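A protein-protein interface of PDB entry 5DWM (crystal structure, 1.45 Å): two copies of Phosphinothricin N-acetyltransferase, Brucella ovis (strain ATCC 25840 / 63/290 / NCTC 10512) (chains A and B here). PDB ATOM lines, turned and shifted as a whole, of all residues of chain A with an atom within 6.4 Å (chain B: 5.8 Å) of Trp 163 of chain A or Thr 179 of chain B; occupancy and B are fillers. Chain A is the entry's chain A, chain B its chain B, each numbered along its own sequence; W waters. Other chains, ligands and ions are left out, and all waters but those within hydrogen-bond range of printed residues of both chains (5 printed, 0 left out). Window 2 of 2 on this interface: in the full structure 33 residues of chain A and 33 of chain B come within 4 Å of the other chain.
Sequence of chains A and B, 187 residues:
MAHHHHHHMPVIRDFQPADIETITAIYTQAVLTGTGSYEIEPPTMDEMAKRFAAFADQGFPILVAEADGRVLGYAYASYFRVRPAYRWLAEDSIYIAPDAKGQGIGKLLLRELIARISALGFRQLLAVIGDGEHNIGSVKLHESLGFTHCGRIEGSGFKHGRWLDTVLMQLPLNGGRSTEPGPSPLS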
ATOM      1  N   ASP A 131      15.882 -15.918  28.493  1.00  0.00           N
ATOM      2  CA  ASP A 131      15.930 -14.856  27.483  1.00  0.00           C
ATOM      3  C   ASP A 131      16.992 -13.811  27.824  1.00  0.00           C
ATOM      4  O   ASP A 131      16.721 -12.608  27.882  1.00  0.00           O
ATOM      5  CB  ASP A 131      14.551 -14.224  27.272  1.00  0.00           C
ATOM      6  CG  ASP A 131      14.499 -13.289  26.065  1.00  0.00           C
ATOM      7  OD1 ASP A 131      15.456 -13.278  25.261  1.00  0.00           O
ATOM      8  OD2 ASP A 131      13.496 -12.562  25.917  1.00  0.00           O
ATOM      9  N   GLY A 155      19.343 -20.738  22.204  1.00  0.00           N
ATOM     10  CA  GLY A 155      18.148 -21.370  21.674  1.00  0.00           C
ATOM     11  C   GLY A 155      17.528 -22.380  22.608  1.00  0.00           C
ATOM     12  O   GLY A 155      16.987 -23.392  22.151  1.00  0.00           O
ATOM     13  N   SER A 156      17.610 -22.140  23.917  1.00  0.00           N
ATOM     14  CA  SER A 156      17.065 -23.062  24.905  1.00  0.00           C
ATOM     15  C   SER A 156      15.548 -22.991  25.015  1.00  0.00           C
ATOM     16  O   SER A 156      14.924 -23.960  25.472  1.00  0.00           O
ATOM     17  CB  SER A 156      17.673 -22.758  26.272  1.00  0.00           C
ATOM     18  OG  SER A 156      17.383 -21.417  26.639  1.00  0.00           O
ATOM     19  N   GLY A 157      14.940 -21.873  24.647  1.00  0.00           N
ATOM     20  CA  GLY A 157      13.503 -21.735  24.760  1.00  0.00           C
ATOM     21  C   GLY A 157      12.905 -21.117  23.516  1.00  0.00           C
ATOM     22  O   GLY A 157      13.563 -20.367  22.789  1.00  0.00           O
ATOM     23  N   PHE A 158      11.641 -21.453  23.264  1.00  0.00           N
ATOM     24  CA  PHE A 158      10.858 -20.783  22.234  1.00  0.00           C
ATOM     25  C   PHE A 158       9.559 -20.329  22.876  1.00  0.00           C
ATOM     26  O   PHE A 158       8.817 -21.155  23.415  1.00  0.00           O
ATOM     27  CB  PHE A 158      10.560 -21.695  21.044  1.00  0.00           C
ATOM     28  CG  PHE A 158       9.963 -20.954  19.893  1.00  0.00           C
ATOM     29  CD1 PHE A 158      10.775 -20.231  19.032  1.00  0.00           C
ATOM     30  CD2 PHE A 158       8.589 -20.934  19.697  1.00  0.00           C
ATOM     31  CE1 PHE A 158      10.228 -19.512  17.981  1.00  0.00           C
ATOM     32  CE2 PHE A 158       8.029 -20.222  18.636  1.00  0.00           C
ATOM     33  CZ  PHE A 158       8.848 -19.514  17.779  1.00  0.00           C
ATOM     34  N   LYS A 159       9.290 -19.027  22.817  1.00  0.00           N
ATOM     35  CA  LYS A 159       8.127 -18.440  23.467  1.00  0.00           C
ATOM     36  C   LYS A 159       7.817 -17.118  22.782  1.00  0.00           C
ATOM     37  O   LYS A 159       8.727 -16.393  22.381  1.00  0.00           O
ATOM     38  CB  LYS A 159       8.389 -18.213  24.966  1.00  0.00           C
ATOM     39  CG  LYS A 159       7.226 -17.586  25.728  1.00  0.00           C
ATOM     40  CD  LYS A 159       7.557 -17.419  27.218  1.00  0.00           C
ATOM     41  CE  LYS A 159       6.381 -16.813  27.953  1.00  0.00           C
ATOM     42  NZ  LYS A 159       6.659 -16.563  29.394  1.00  0.00           N
ATOM     43  N   GLY A 161       6.860 -16.485  19.914  1.00  0.00           N
ATOM     44  CA  GLY A 161       7.357 -16.439  18.552  1.00  0.00           C
ATOM     45  C   GLY A 161       8.845 -16.214  18.398  1.00  0.00           C
ATOM     46  O   GLY A 161       9.297 -15.957  17.277  1.00  0.00           O
ATOM     47  N   ARG A 162       9.628 -16.330  19.474  1.00  0.00           N
ATOM     48  CA  ARG A 162      11.047 -16.003  19.451  1.00  0.00           C
ATOM     49  C   ARG A 162      11.857 -17.100  20.120  1.00  0.00           C
ATOM     50  O   ARG A 162      11.437 -17.663  21.138  1.00  0.00           O
ATOM     51  CB  ARG A 162      11.334 -14.699  20.232  1.00  0.00           C
ATOM     52  CG  ARG A 162      11.160 -13.409  19.464  1.00  0.00           C
ATOM     53  CD  ARG A 162      11.940 -12.265  20.134  1.00  0.00           C
ATOM     54  NE  ARG A 162      11.588 -12.100  21.545  1.00  0.00           N
ATOM     55  CZ  ARG A 162      12.432 -12.222  22.572  1.00  0.00           C
ATOM     56  NH1 ARG A 162      13.714 -12.510  22.377  1.00  0.00           N
ATOM     57  NH2 ARG A 162      11.991 -12.043  23.807  1.00  0.00           N
ATOM     58  N   TRP A 163      13.033 -17.378  19.563  1.00  0.00           N
ATOM     59  CA  TRP A 163      14.003 -18.227  20.241  1.00  0.00           C
ATOM     60  C   TRP A 163      14.715 -17.427  21.323  1.00  0.00           C
ATOM     61  O   TRP A 163      15.037 -16.248  21.135  1.00  0.00           O
ATOM     62  CB  TRP A 163      15.024 -18.798  19.255  1.00  0.00           C
ATOM     63  CG  TRP A 163      14.463 -19.909  18.425  1.00  0.00           C
ATOM     64  CD1 TRP A 163      14.106 -19.853  17.105  1.00  0.00           C
ATOM     65  CD2 TRP A 163      14.191 -21.246  18.863  1.00  0.00           C
ATOM     66  NE1 TRP A 163      13.635 -21.088  16.693  1.00  0.00           N
ATOM     67  CE2 TRP A 163      13.673 -21.954  17.757  1.00  0.00           C
ATOM     68  CE3 TRP A 163      14.337 -21.910  20.088  1.00  0.00           C
ATOM     69  CZ2 TRP A 163      13.296 -23.290  17.841  1.00  0.00           C
ATOM     70  CZ3 TRP A 163      13.966 -23.234  20.173  1.00  0.00           C
ATOM     71  CH2 TRP A 163      13.449 -23.914  19.058  1.00  0.00           C
ATOM     72  N   LEU A 164      14.966 -18.082  22.454  1.00  0.00           N
ATOM     73  CA  LEU A 164      15.485 -17.435  23.649  1.00  0.00           C
ATOM     74  C   LEU A 164      16.740 -18.166  24.087  1.00  0.00           C
ATOM     75  O   LEU A 164      16.832 -19.385  23.939  1.00  0.00           O
ATOM     76  CB  LEU A 164      14.475 -17.547  24.792  1.00  0.00           C
ATOM     77  CG  LEU A 164      13.013 -17.221  24.466  1.00  0.00           C
ATOM     78  CD1 LEU A 164      12.135 -17.454  25.693  1.00  0.00           C
ATOM     79  CD2 LEU A 164      12.868 -15.792  23.958  1.00  0.00           C
ATOM     80  N   ASP A 165      17.689 -17.423  24.658  1.00  0.00           N
ATOM     81  CA  ASP A 165      18.903 -18.003  25.214  1.00  0.00           C
ATOM     82  C   ASP A 165      18.826 -17.987  26.732  1.00  0.00           C
ATOM     83  O   ASP A 165      18.239 -17.080  27.322  1.00  0.00           O
ATOM     84  CB  ASP A 165      20.149 -17.202  24.815  1.00  0.00           C
ATOM     85  CG  ASP A 165      20.404 -17.191  23.314  1.00  0.00           C
ATOM     86  OD1 ASP A 165      19.774 -17.960  22.561  1.00  0.00           O
ATOM     87  OD2 ASP A 165      21.260 -16.398  22.880  1.00  0.00           O
ATOM     88  N   ALA B  85       8.548 -23.815  27.415  1.00  0.00           N
ATOM     89  CA  ALA B  85       9.406 -23.179  26.420  1.00  0.00           C
ATOM     90  C   ALA B  85      10.671 -23.978  26.142  1.00  0.00           C
ATOM     91  O   ALA B  85      11.287 -23.782  25.092  1.00  0.00           O
ATOM     92  CB  ALA B  85       9.727 -21.725  26.785  1.00  0.00           C
ATOM     93  N   TRP B  88      11.948 -27.933  23.079  1.00  0.00           N
ATOM     94  CA  TRP B  88      12.798 -28.281  21.946  1.00  0.00           C
ATOM     95  C   TRP B  88      14.242 -28.541  22.362  1.00  0.00           C
ATOM     96  O   TRP B  88      15.109 -28.698  21.494  1.00  0.00           O
ATOM     97  CB  TRP B  88      12.728 -27.209  20.851  1.00  0.00           C
ATOM     98  CG  TRP B  88      11.385 -27.110  20.190  1.00  0.00           C
ATOM     99  CD1 TRP B  88      11.001 -27.695  19.011  1.00  0.00           C
ATOM    100  CD2 TRP B  88      10.252 -26.368  20.656  1.00  0.00           C
ATOM    101  NE1 TRP B  88       9.699 -27.376  18.734  1.00  0.00           N
ATOM    102  CE2 TRP B  88       9.220 -26.548  19.717  1.00  0.00           C
ATOM    103  CE3 TRP B  88      10.014 -25.561  21.774  1.00  0.00           C
ATOM    104  CZ2 TRP B  88       7.963 -25.952  19.863  1.00  0.00           C
ATOM    105  CZ3 TRP B  88       8.772 -24.982  21.926  1.00  0.00           C
ATOM    106  CH2 TRP B  88       7.762 -25.173  20.972  1.00  0.00           C
ATOM    107  N   ARG B 123      15.575 -29.213  18.696  1.00  0.00           N
ATOM    108  CA  ARG B 123      16.429 -28.215  18.067  1.00  0.00           C
ATOM    109  C   ARG B 123      17.788 -28.049  18.729  1.00  0.00           C
ATOM    110  O   ARG B 123      18.687 -27.472  18.110  1.00  0.00           O
ATOM    111  CB  ARG B 123      15.732 -26.844  18.027  1.00  0.00           C
ATOM    112  CG  ARG B 123      14.480 -26.799  17.149  1.00  0.00           C
ATOM    113  CD  ARG B 123      14.800 -27.239  15.722  1.00  0.00           C
ATOM    114  NE  ARG B 123      13.698 -27.028  14.789  1.00  0.00           N
ATOM    115  CZ  ARG B 123      13.423 -25.857  14.228  1.00  0.00           C
ATOM    116  NH1 ARG B 123      14.174 -24.790  14.510  1.00  0.00           N
ATOM    117  NH2 ARG B 123      12.401 -25.746  13.384  1.00  0.00           N
ATOM    118  N   ASN B 174      18.224 -29.879  13.375  1.00  0.00           N
ATOM    119  CA  ASN B 174      17.067 -29.440  12.577  1.00  0.00           C
ATOM    120  C   ASN B 174      17.028 -27.924  12.389  1.00  0.00           C
ATOM    121  O   ASN B 174      15.956 -27.313  12.379  1.00  0.00           O
ATOM    122  CB  ASN B 174      15.745 -29.916  13.187  1.00  0.00           C
ATOM    123  CG  ASN B 174      15.609 -31.420  13.192  1.00  0.00           C
ATOM    124  OD1 ASN B 174      15.695 -32.064  12.136  1.00  0.00           O
ATOM    125  ND2 ASN B 174      15.404 -31.998  14.376  1.00  0.00           N
ATOM    126  N   GLY B 175      18.202 -27.305  12.259  1.00  0.00           N
ATOM    127  CA  GLY B 175      18.278 -25.870  12.066  1.00  0.00           C
ATOM    128  C   GLY B 175      18.470 -25.051  13.332  1.00  0.00           C
ATOM    129  O   GLY B 175      18.647 -23.828  13.237  1.00  0.00           O
ATOM    130  N   GLY B 176      18.447 -25.674  14.511  1.00  0.00           N
ATOM    131  CA  GLY B 176      18.729 -24.929  15.730  1.00  0.00           C
ATOM    132  C   GLY B 176      17.720 -23.813  15.956  1.00  0.00           C
ATOM    133  O   GLY B 176      16.506 -24.036  15.968  1.00  0.00           O
ATOM    134  N   ARG B 177      18.218 -22.593  16.154  1.00  0.00           N
ATOM    135  CA  ARG B 177      17.345 -21.437  16.323  1.00  0.00           C
ATOM    136  C   ARG B 177      17.182 -20.619  15.040  1.00  0.00           C
ATOM    137  O   ARG B 177      16.731 -19.472  15.097  1.00  0.00           O
ATOM    138  CB  ARG B 177      17.784 -20.571  17.510  1.00  0.00           C
ATOM    139  CG  ARG B 177      19.230 -20.069  17.500  1.00  0.00           C
ATOM    140  CD  ARG B 177      19.413 -18.964  18.555  1.00  0.00           C
ATOM    141  NE  ARG B 177      18.629 -17.780  18.205  1.00  0.00           N
ATOM    142  CZ  ARG B 177      18.175 -16.865  19.059  1.00  0.00           C
ATOM    143  NH1 ARG B 177      18.408 -16.961  20.360  1.00  0.00           N
ATOM    144  NH2 ARG B 177      17.468 -15.846  18.598  1.00  0.00           N
ATOM    145  N   SER B 178      17.503 -21.193  13.882  1.00  0.00           N
ATOM    146  CA  SER B 178      17.470 -20.416  12.650  1.00  0.00           C
ATOM    147  C   SER B 178      16.117 -20.446  11.949  1.00  0.00           C
ATOM    148  O   SER B 178      15.930 -19.700  10.981  1.00  0.00           O
ATOM    149  CB  SER B 178      18.559 -20.887  11.683  1.00  0.00           C
ATOM    150  OG  SER B 178      18.224 -22.156  11.150  1.00  0.00           O
ATOM    151  N   THR B 179      15.180 -21.286  12.397  1.00  0.00           N
ATOM    152  CA  THR B 179      13.831 -21.309  11.848  1.00  0.00           C
ATOM    153  C   THR B 179      12.821 -21.415  12.978  1.00  0.00           C
ATOM    154  O   THR B 179      13.121 -21.954  14.048  1.00  0.00           O
ATOM    155  CB  THR B 179      13.588 -22.502  10.904  1.00  0.00           C
ATOM    156  OG1 THR B 179      13.654 -23.724  11.650  1.00  0.00           O
ATOM    157  CG2 THR B 179      14.602 -22.523   9.765  1.00  0.00           C
ATOM    158  N   GLU B 180      11.611 -20.907  12.726  1.00  0.00           N
ATOM    159  CA  GLU B 180      10.526 -21.118  13.672  1.00  0.00           C
ATOM    160  C   GLU B 180      10.161 -22.601  13.705  1.00  0.00           C
ATOM    161  O   GLU B 180      10.104 -23.251  12.658  1.00  0.00           O
ATOM    162  CB  GLU B 180       9.299 -20.279  13.297  1.00  0.00           C
ATOM    163  CG  GLU B 180       9.537 -18.768  13.402  1.00  0.00           C
ATOM    164  CD  GLU B 180       8.393 -17.921  12.838  1.00  0.00           C
ATOM    165  OE1 GLU B 180       8.594 -16.700  12.661  1.00  0.00           O
ATOM    166  OE2 GLU B 180       7.296 -18.464  12.565  1.00  0.00           O
ATOM    167  N   PRO B 181       9.923 -23.163  14.883  1.00  0.00           N
ATOM    168  CA  PRO B 181       9.599 -24.588  14.985  1.00  0.00           C
ATOM    169  C   PRO B 181       8.121 -24.852  14.717  1.00  0.00           C
ATOM    170  O   PRO B 181       7.289 -23.944  14.674  1.00  0.00           O
ATOM    171  CB  PRO B 181       9.931 -24.894  16.448  1.00  0.00           C
ATOM    172  CG  PRO B 181       9.581 -23.616  17.161  1.00  0.00           C
ATOM    173  CD  PRO B 181       9.995 -22.509  16.205  1.00  0.00           C
HETATM  174  O   HOH W   1       7.722 -15.312  15.239  1.00  0.00           O
HETATM  175  O   HOH W   2      17.120 -23.710  19.213  1.00  0.00           O
HETATM  176  O   HOH W   3      15.770 -25.776  22.596  1.00  0.00           O
HETATM  177  O   HOH W   4      13.115 -25.380  23.582  1.00  0.00           O
HETATM  178  O   HOH W   5      17.730 -14.427  21.824  1.00  0.00           O
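No position is printed for both chains.
Among the printed residues, merely in contact across the chains: Gly 157 of chain A with Ala 85 of chain B (3.0 Å), Trp 163 of chain A with Arg 177 of chain B (3.3 Å), Phe 158 of chain A with Pro 181 of chain B (3.5 Å), Trp 163 of chain A with Arg 123 of chain B (3.6 Å), Ser 156 of chain A with Ala 85 of chain B (3.7 Å), Trp 163 of chain A with Pro 181 of chain B (3.8 Å), Trp 163 of chain A with Gly 176 of chain B (3.8 Å), Trp 163 of chain A with Trp 88 of chain B (3.8 Å) and Phe 158 of chain A with Trp 88 of chain B (3.8 Å).
Water W1 lies within hydrogen-bond range of O of Gly 161 of chain A (2.7 Å) and OE1 of Glu 180 of chain B (3.1 Å).
Water W3 bridges the backbone carbonyl oxygen (O) of Gly 155 of chain A (2.7 Å) and the backbone carbonyl oxygen (O) of Trp 88 of chain B (3.2 Å).
Water W4 lies within hydrogen-bond range of the backbone NH of Trp 88 of chain B, the backbone carbonyl oxygen of Ala 85 of chain B and the backbone carbonyl oxygen of Ser 156 of chain A.
Water W2 lies within hydrogen-bond range of the backbone carbonyl oxygen (O) of Gly 155 of chain A (3.0 Å), the backbone carbonyl oxygen (O) of Gly 176 of chain B (3.3 Å) and the backbone NH (N) of Arg 177 of chain B (3.4 Å).
Water W5 lies within hydrogen-bond range of NH1 of Arg 177 of chain B (3.0 Å) and O of Trp 163 of chain A (3.3 Å).
Printed residues of chain B that touch a printed residue of chain A: Ala 85, Trp 88, Arg 123, Gly 176, Arg 177, Thr 179 and Pro 181.
Hydrophobic or aromatic side chains of chain B that line the printed part of chain A: Ala 85, Trp 88 and Pro 181.
Printed residues of chain A that touch a printed residue of chain B: Ser 156, Gly 157, Phe 158, Trp 163 and Asp 165.
Of the printed residues of chain B, Ser 156 of chain A touches Ala 85 (3.7 Å).
Printed residues of chain B within 4 Å of Gly 157 of chain A: Ala 85 (3.0 Å).
Of the printed residues of chain A, Trp 88 of chain B touches Phe 158 (3.8 Å) and Trp 163 (3.8 Å).
Of the printed residues of chain A, Arg 123 of chain B touches Trp 163.
Of the printed residues of chain A, Gly 176 of chain B touches Trp 163.
Thr 179 of chain B touches just one residue of chain A: Trp 163 (2.8 Å).
The nearest residue of chain A that does not touch Thr 179 of chain B is Phe 158 of chain A (5.5 Å).
O of Ala 85 of chain B sits at hydrogen-bond distance from N of Phe 158 of chain A (3.0 Å).
NE1 of Trp 163 of chain A sits at hydrogen-bond distance from O of Thr 179 of chain B, 2.8 Å away.
The side-chain carboxylate (OD1) of Asp 165 of chain A is in salt-bridge range of the guanidinium group (NH1) of Arg 177 of chain B (2.8 Å).
The backbone NH (N) of Asp 131 of chain A is in hydrogen-bond range of the backbone carbonyl oxygen (O) of Asp 165 of chain A (2.9 Å).
The backbone NH (N) of Gly 155 of chain A is in hydrogen-bond range of the side-chain carboxylate (OD1) of Asp 165 of chain A, 2.8 Å away.
The backbone carbonyl oxygen (O) of Leu 164 of chain A sits at hydrogen-bond distance from the backbone NH (N) of Ser 156 of chain A, at 2.9 Å.
The guanidinium group of Arg 123 of chain B sits at hydrogen-bond distance from the side-chain hydroxyl of Thr 179 of chain B (2.9 Å).
The guanidinium group of Arg 123 of chain B lies within hydrogen-bond range of the backbone carbonyl oxygen of Asn 174 of chain B.
O of Gly 157 of chain A is in hydrogen-bond range of N of Leu 164 of chain A (2.7 Å).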
